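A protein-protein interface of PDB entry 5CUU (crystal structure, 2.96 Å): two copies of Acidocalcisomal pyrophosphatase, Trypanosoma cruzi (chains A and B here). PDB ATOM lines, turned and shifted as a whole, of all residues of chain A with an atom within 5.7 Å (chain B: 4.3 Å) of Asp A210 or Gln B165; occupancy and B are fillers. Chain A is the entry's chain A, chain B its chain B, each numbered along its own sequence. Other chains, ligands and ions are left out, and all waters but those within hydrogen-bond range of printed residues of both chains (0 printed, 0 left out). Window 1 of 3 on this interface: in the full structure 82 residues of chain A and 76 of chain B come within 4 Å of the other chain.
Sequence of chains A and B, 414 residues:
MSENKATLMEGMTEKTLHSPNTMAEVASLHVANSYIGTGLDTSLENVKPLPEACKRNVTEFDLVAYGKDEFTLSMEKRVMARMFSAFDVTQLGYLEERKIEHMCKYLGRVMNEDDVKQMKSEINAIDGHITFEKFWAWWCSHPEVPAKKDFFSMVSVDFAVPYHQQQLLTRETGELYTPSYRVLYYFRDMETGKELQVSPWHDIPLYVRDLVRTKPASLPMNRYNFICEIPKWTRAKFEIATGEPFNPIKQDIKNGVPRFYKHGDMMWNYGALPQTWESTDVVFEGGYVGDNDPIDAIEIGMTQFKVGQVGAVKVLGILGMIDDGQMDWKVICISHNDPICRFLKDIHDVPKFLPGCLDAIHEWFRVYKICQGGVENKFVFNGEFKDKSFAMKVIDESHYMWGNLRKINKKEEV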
ATOM      1  N   PHE A 159     -18.937   7.174 -20.675  1.00  0.00           N
ATOM      2  CA  PHE A 159     -18.512   6.518 -21.907  1.00  0.00           C
ATOM      3  C   PHE A 159     -19.711   5.649 -22.299  1.00  0.00           C
ATOM      4  O   PHE A 159     -19.691   4.418 -22.207  1.00  0.00           O
ATOM      5  CB  PHE A 159     -17.257   5.679 -21.594  1.00  0.00           C
ATOM      6  CG  PHE A 159     -16.780   4.780 -22.716  1.00  0.00           C
ATOM      7  CD1 PHE A 159     -16.518   5.281 -23.986  1.00  0.00           C
ATOM      8  CD2 PHE A 159     -16.480   3.439 -22.454  1.00  0.00           C
ATOM      9  CE1 PHE A 159     -15.957   4.455 -24.963  1.00  0.00           C
ATOM     10  CE2 PHE A 159     -15.923   2.618 -23.425  1.00  0.00           C
ATOM     11  CZ  PHE A 159     -15.658   3.123 -24.675  1.00  0.00           C
ATOM     12  N   VAL A 208     -11.149 -10.596 -30.927  1.00  0.00           N
ATOM     13  CA  VAL A 208     -12.154 -10.573 -29.897  1.00  0.00           C
ATOM     14  C   VAL A 208     -11.770  -9.483 -28.931  1.00  0.00           C
ATOM     15  O   VAL A 208     -10.911  -9.668 -28.090  1.00  0.00           O
ATOM     16  CB  VAL A 208     -12.259 -11.886 -29.152  1.00  0.00           C
ATOM     17  CG1 VAL A 208     -13.143 -11.709 -27.911  1.00  0.00           C
ATOM     18  CG2 VAL A 208     -12.880 -12.915 -30.053  1.00  0.00           C
ATOM     19  N   ARG A 209     -12.396  -8.329 -29.056  1.00  0.00           N
ATOM     20  CA  ARG A 209     -12.051  -7.260 -28.157  1.00  0.00           C
ATOM     21  C   ARG A 209     -13.128  -6.950 -27.143  1.00  0.00           C
ATOM     22  O   ARG A 209     -14.295  -7.246 -27.378  1.00  0.00           O
ATOM     23  CB  ARG A 209     -11.672  -6.014 -28.963  1.00  0.00           C
ATOM     24  CG  ARG A 209     -10.239  -6.079 -29.556  1.00  0.00           C
ATOM     25  CD  ARG A 209      -9.950  -4.897 -30.498  1.00  0.00           C
ATOM     26  NE  ARG A 209      -8.637  -5.013 -31.142  1.00  0.00           N
ATOM     27  CZ  ARG A 209      -8.334  -4.506 -32.338  1.00  0.00           C
ATOM     28  NH1 ARG A 209      -9.251  -3.838 -33.051  1.00  0.00           N
ATOM     29  NH2 ARG A 209      -7.102  -4.666 -32.819  1.00  0.00           N
ATOM     30  N   ASP A 210     -12.704  -6.397 -26.001  1.00  0.00           N
ATOM     31  CA  ASP A 210     -13.583  -6.007 -24.885  1.00  0.00           C
ATOM     32  C   ASP A 210     -13.791  -4.507 -24.834  1.00  0.00           C
ATOM     33  O   ASP A 210     -12.828  -3.758 -24.934  1.00  0.00           O
ATOM     34  CB  ASP A 210     -12.986  -6.439 -23.555  1.00  0.00           C
ATOM     35  CG  ASP A 210     -13.081  -7.909 -23.360  1.00  0.00           C
ATOM     36  OD1 ASP A 210     -14.234  -8.409 -23.510  1.00  0.00           O
ATOM     37  OD2 ASP A 210     -12.026  -8.549 -23.073  1.00  0.00           O
ATOM     38  N   LEU A 211     -15.029  -4.057 -24.677  1.00  0.00           N
ATOM     39  CA  LEU A 211     -15.243  -2.624 -24.631  1.00  0.00           C
ATOM     40  C   LEU A 211     -14.295  -2.019 -23.624  1.00  0.00           C
ATOM     41  O   LEU A 211     -13.673  -1.005 -23.911  1.00  0.00           O
ATOM     42  CB  LEU A 211     -16.683  -2.271 -24.256  1.00  0.00           C
ATOM     43  CG  LEU A 211     -17.433  -1.478 -25.337  1.00  0.00           C
ATOM     44  CD1 LEU A 211     -16.415  -0.722 -26.260  1.00  0.00           C
ATOM     45  CD2 LEU A 211     -18.287  -2.450 -26.177  1.00  0.00           C
ATOM     46  N   VAL A 212     -14.193  -2.641 -22.443  1.00  0.00           N
ATOM     47  CA  VAL A 212     -13.276  -2.197 -21.373  1.00  0.00           C
ATOM     48  C   VAL A 212     -12.494  -3.457 -21.039  1.00  0.00           C
ATOM     49  O   VAL A 212     -13.084  -4.441 -20.641  1.00  0.00           O
ATOM     50  CB  VAL A 212     -14.020  -1.661 -20.082  1.00  0.00           C
ATOM     51  CG1 VAL A 212     -13.046  -1.212 -19.071  1.00  0.00           C
ATOM     52  CG2 VAL A 212     -14.900  -0.500 -20.402  1.00  0.00           C
ATOM     53  N   ARG A 213     -11.182  -3.413 -21.263  1.00  0.00           N
ATOM     54  CA  ARG A 213     -10.279  -4.529 -21.030  1.00  0.00           C
ATOM     55  C   ARG A 213      -9.839  -4.458 -19.599  1.00  0.00           C
ATOM     56  O   ARG A 213      -9.301  -3.440 -19.162  1.00  0.00           O
ATOM     57  CB  ARG A 213      -9.048  -4.435 -21.953  1.00  0.00           C
ATOM     58  CG  ARG A 213      -8.082  -5.670 -21.915  1.00  0.00           C
ATOM     59  CD  ARG A 213      -7.864  -6.361 -23.320  1.00  0.00           C
ATOM     60  NE  ARG A 213      -7.006  -7.536 -23.221  1.00  0.00           N
ATOM     61  CZ  ARG A 213      -5.787  -7.497 -22.689  1.00  0.00           C
ATOM     62  NH1 ARG A 213      -5.294  -6.345 -22.237  1.00  0.00           N
ATOM     63  NH2 ARG A 213      -5.093  -8.619 -22.535  1.00  0.00           N
ATOM     64  N   THR A 214     -10.066  -5.542 -18.866  1.00  0.00           N
ATOM     65  CA  THR A 214      -9.714  -5.567 -17.467  1.00  0.00           C
ATOM     66  C   THR A 214      -8.500  -6.413 -17.190  1.00  0.00           C
ATOM     67  O   THR A 214      -7.917  -6.316 -16.099  1.00  0.00           O
ATOM     68  CB  THR A 214     -10.924  -5.970 -16.588  1.00  0.00           C
ATOM     69  OG1 THR A 214     -11.786  -6.890 -17.276  1.00  0.00           O
ATOM     70  CG2 THR A 214     -11.728  -4.728 -16.256  1.00  0.00           C
ATOM     71  N   LYS A 215      -8.084  -7.204 -18.185  1.00  0.00           N
ATOM     72  CA  LYS A 215      -6.874  -8.016 -18.046  1.00  0.00           C
ATOM     73  C   LYS A 215      -5.728  -7.026 -17.975  1.00  0.00           C
ATOM     74  O   LYS A 215      -5.718  -6.028 -18.688  1.00  0.00           O
ATOM     75  CB  LYS A 215      -6.661  -8.885 -19.256  1.00  0.00           C
ATOM     76  CG  LYS A 215      -7.776  -9.808 -19.542  1.00  0.00           C
ATOM     77  CD  LYS A 215      -7.451 -10.700 -20.719  1.00  0.00           C
ATOM     78  CE  LYS A 215      -8.453 -11.860 -20.803  1.00  0.00           C
ATOM     79  NZ  LYS A 215      -8.087 -13.012 -19.910  1.00  0.00           N
ATOM     80  N   MET A 221      -2.633  -8.412 -25.927  1.00  0.00           N
ATOM     81  CA  MET A 221      -3.868  -8.996 -26.423  1.00  0.00           C
ATOM     82  C   MET A 221      -3.746 -10.197 -27.343  1.00  0.00           C
ATOM     83  O   MET A 221      -3.170 -10.117 -28.434  1.00  0.00           O
ATOM     84  CB  MET A 221      -4.708  -7.932 -27.102  1.00  0.00           C
ATOM     85  CG  MET A 221      -5.008  -6.746 -26.227  1.00  0.00           C
ATOM     86  SD  MET A 221      -6.107  -5.563 -27.080  1.00  0.00           S
ATOM     87  CE  MET A 221      -7.718  -6.773 -27.512  1.00  0.00           C
ATOM     88  N   TYR B 163     -16.694   2.685 -31.021  1.00  0.00           N
ATOM     89  CA  TYR B 163     -16.171   2.546 -29.674  1.00  0.00           C
ATOM     90  C   TYR B 163     -14.713   2.114 -29.643  1.00  0.00           C
ATOM     91  O   TYR B 163     -14.321   1.166 -30.316  1.00  0.00           O
ATOM     92  CB  TYR B 163     -17.078   1.579 -28.910  1.00  0.00           C
ATOM     93  CG  TYR B 163     -18.529   2.047 -28.978  1.00  0.00           C
ATOM     94  CD1 TYR B 163     -18.831   3.408 -28.845  1.00  0.00           C
ATOM     95  CD2 TYR B 163     -19.589   1.157 -29.194  1.00  0.00           C
ATOM     96  CE1 TYR B 163     -20.138   3.878 -28.922  1.00  0.00           C
ATOM     97  CE2 TYR B 163     -20.913   1.623 -29.272  1.00  0.00           C
ATOM     98  CZ  TYR B 163     -21.172   2.992 -29.134  1.00  0.00           C
ATOM     99  OH  TYR B 163     -22.447   3.516 -29.203  1.00  0.00           O
ATOM    100  N   HIS B 164     -13.900   2.858 -28.902  1.00  0.00           N
ATOM    101  CA  HIS B 164     -12.478   2.549 -28.768  1.00  0.00           C
ATOM    102  C   HIS B 164     -12.260   1.656 -27.535  1.00  0.00           C
ATOM    103  O   HIS B 164     -12.431   2.096 -26.390  1.00  0.00           O
ATOM    104  CB  HIS B 164     -11.633   3.824 -28.583  1.00  0.00           C
ATOM    105  CG  HIS B 164     -11.747   4.825 -29.693  1.00  0.00           C
ATOM    106  ND1 HIS B 164     -10.909   5.918 -29.788  1.00  0.00           N
ATOM    107  CD2 HIS B 164     -12.633   4.941 -30.711  1.00  0.00           C
ATOM    108  CE1 HIS B 164     -11.278   6.667 -30.812  1.00  0.00           C
ATOM    109  NE2 HIS B 164     -12.321   6.097 -31.389  1.00  0.00           N
ATOM    110  N   GLN B 165     -11.895   0.403 -27.767  1.00  0.00           N
ATOM    111  CA  GLN B 165     -11.649  -0.483 -26.653  1.00  0.00           C
ATOM    112  C   GLN B 165     -10.782   0.309 -25.683  1.00  0.00           C
ATOM    113  O   GLN B 165      -9.857   0.996 -26.102  1.00  0.00           O
ATOM    114  CB  GLN B 165     -10.938  -1.742 -27.141  1.00  0.00           C
ATOM    115  CG  GLN B 165     -10.342  -2.566 -26.048  1.00  0.00           C
ATOM    116  CD  GLN B 165      -9.861  -3.890 -26.561  1.00  0.00           C
ATOM    117  OE1 GLN B 165      -9.180  -3.968 -27.594  1.00  0.00           O
ATOM    118  NE2 GLN B 165     -10.208  -4.955 -25.847  1.00  0.00           N
ATOM    119  N   GLN B 166     -11.106   0.250 -24.394  1.00  0.00           N
ATOM    120  CA  GLN B 166     -10.335   0.982 -23.392  1.00  0.00           C
ATOM    121  C   GLN B 166      -9.579  -0.007 -22.546  1.00  0.00           C
ATOM    122  O   GLN B 166     -10.037  -1.120 -22.344  1.00  0.00           O
ATOM    123  CB  GLN B 166     -11.249   1.808 -22.472  1.00  0.00           C
ATOM    124  CG  GLN B 166     -12.171   2.795 -23.170  1.00  0.00           C
ATOM    125  CD  GLN B 166     -11.437   3.937 -23.805  1.00  0.00           C
ATOM    126  OE1 GLN B 166     -11.653   4.257 -24.967  1.00  0.00           O
ATOM    127  NE2 GLN B 166     -10.572   4.580 -23.039  1.00  0.00           N
ATOM    128  N   ARG B 188      -7.205   3.747 -20.821  1.00  0.00           N
ATOM    129  CA  ARG B 188      -6.211   4.188 -21.760  1.00  0.00           C
ATOM    130  C   ARG B 188      -6.851   3.800 -23.059  1.00  0.00           C
ATOM    131  O   ARG B 188      -7.207   2.646 -23.276  1.00  0.00           O
ATOM    132  CB  ARG B 188      -4.878   3.474 -21.578  1.00  0.00           C
ATOM    133  CG  ARG B 188      -3.780   4.030 -22.468  1.00  0.00           C
ATOM    134  CD  ARG B 188      -2.571   3.166 -22.378  1.00  0.00           C
ATOM    135  NE  ARG B 188      -1.762   3.391 -21.180  1.00  0.00           N
ATOM    136  CZ  ARG B 188      -1.046   2.432 -20.572  1.00  0.00           C
ATOM    137  NH1 ARG B 188      -0.317   2.712 -19.494  1.00  0.00           N
ATOM    138  NH2 ARG B 188      -1.079   1.177 -21.026  1.00  0.00           N
ATOM    139  N   ASP B 189      -7.065   4.810 -23.884  1.00  0.00           N
ATOM    140  CA  ASP B 189      -7.666   4.643 -25.194  1.00  0.00           C
ATOM    141  C   ASP B 189      -6.681   3.774 -25.968  1.00  0.00           C
ATOM    142  O   ASP B 189      -5.503   4.143 -26.116  1.00  0.00           O
ATOM    143  CB  ASP B 189      -7.800   6.022 -25.832  1.00  0.00           C
ATOM    144  CG  ASP B 189      -8.771   6.043 -26.967  1.00  0.00           C
ATOM    145  OD1 ASP B 189      -8.637   5.182 -27.871  1.00  0.00           O
ATOM    146  OD2 ASP B 189      -9.659   6.932 -26.949  1.00  0.00           O
ATOM    147  N   MET B 190      -7.128   2.610 -26.436  1.00  0.00           N
ATOM    148  CA  MET B 190      -6.223   1.727 -27.167  1.00  0.00           C
ATOM    149  C   MET B 190      -6.112   2.096 -28.640  1.00  0.00           C
ATOM    150  O   MET B 190      -5.691   1.264 -29.448  1.00  0.00           O
ATOM    151  CB  MET B 190      -6.659   0.288 -27.038  1.00  0.00           C
ATOM    152  CG  MET B 190      -6.506  -0.231 -25.681  1.00  0.00           C
ATOM    153  SD  MET B 190      -7.078  -1.942 -25.582  1.00  0.00           S
ATOM    154  CE  MET B 190      -5.435  -2.880 -25.224  1.00  0.00           C
ATOM    155  N   VAL B 208     -19.845  -8.013 -18.750  1.00  0.00           N
ATOM    156  CA  VAL B 208     -18.759  -8.107 -19.706  1.00  0.00           C
ATOM    157  C   VAL B 208     -19.440  -8.735 -20.932  1.00  0.00           C
ATOM    158  O   VAL B 208     -19.754  -9.915 -20.950  1.00  0.00           O
ATOM    159  CB  VAL B 208     -17.638  -9.068 -19.204  1.00  0.00           C
ATOM    160  CG1 VAL B 208     -16.429  -9.071 -20.176  1.00  0.00           C
ATOM    161  CG2 VAL B 208     -17.193  -8.649 -17.822  1.00  0.00           C
ATOM    162  N   ASP B 210     -19.667  -9.413 -25.248  1.00  0.00           N
ATOM    163  CA  ASP B 210     -18.864  -9.500 -26.456  1.00  0.00           C
ATOM    164  C   ASP B 210     -19.630  -8.931 -27.641  1.00  0.00           C
ATOM    165  O   ASP B 210     -20.779  -9.325 -27.848  1.00  0.00           O
ATOM    166  CB  ASP B 210     -18.513 -10.961 -26.741  1.00  0.00           C
ATOM    167  CG  ASP B 210     -17.309 -11.422 -25.962  1.00  0.00           C
ATOM    168  OD1 ASP B 210     -16.270 -10.698 -26.007  1.00  0.00           O
ATOM    169  OD2 ASP B 210     -17.408 -12.497 -25.316  1.00  0.00           O
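Val A208 touches Asp B210, but with the chains exchanged Asp A210 does not touch Val B208 (4.05 Å). Asp B210 touches its own counterpart, Asp A210.
The backbone NH of Asp A210 lies close to the side-chain amide nitrogen of Gln B165 (2.9 Å). O of Leu A211 lies within hydrogen-bond range of N of Gln B166. N of Arg A213 sits at hydrogen-bond distance from O of Gln B166 (2.8 Å). The side-chain sulfur of Met A221 sits close to the side-chain amide oxygen of Gln B165 (3.5 Å).
O of His B164 lies close to OE1 of Gln B166, 2.7 Å away. The side-chain carboxylate of Asp B189 sits at hydrogen-bond distance from a ring nitrogen (ND1) of His B164, at 3.1 Å. The backbone carbonyl oxygen (O) of Gln B165 sits at hydrogen-bond distance from the backbone NH (N) of Met B190 (3.2 Å).
Among the printed residues, pairs that only touch across the chains: Arg A209 with Gln B165 (3.1 Å), Met A221 with Met B190 (3.3 Å), Leu A211 with Gln B165 (3.4 Å), Val A212 with Gln B166 (3.5 Å), Leu A211 with Tyr B163 (3.6 Å), Arg A213 with Gln B165 (3.7 Å), Phe A159 with Gln B166 (3.8 Å), Phe A159 with His B164 (3.8 Å), Val A208 with Asp B210 (3.8 Å) and Asp A210 with Asp B210 (3.95 Å).
Printed residues of chain B that touch a printed residue of chain A: Tyr B163, His B164, Gln B165, Gln B166, Met B190 and Asp B210. Among the printed residues, 14 pairs touch across the chains. Among the printed residues, no Asp or Glu carboxylate lies within 4 Å of a Lys or Arg side-chain nitrogen of the other chain.
Of chain B, only Gln B165 (2.9 Å) and Asp B210 (3.95 Å) come within 4 Å of Asp A210. Of the printed residues of chain A, Gln B166 touches Phe A159, Leu A211, Val A212 and Arg A213. Printed residues of chain B within 4 Å of Phe A159: His B164 (3.8 Å) and Gln B166 (3.8 Å). Printed residues of chain B within 4 Å of Arg A213: Gln B165 (3.7 Å) and Gln B166 (2.8 Å). Printed residues of chain B within 4 Å of Met A221: Gln B165 and Met B190. Of the printed residues of chain B, Leu A211 touches Tyr B163 (3.6 Å), Gln B165 (3.4 Å) and Gln B166 (2.9 Å). Asp B189 touches none of the printed residues of chain A. The nearest printed residue of chain A that does not touch Gln B165 is Val A208 (5.3 Å).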
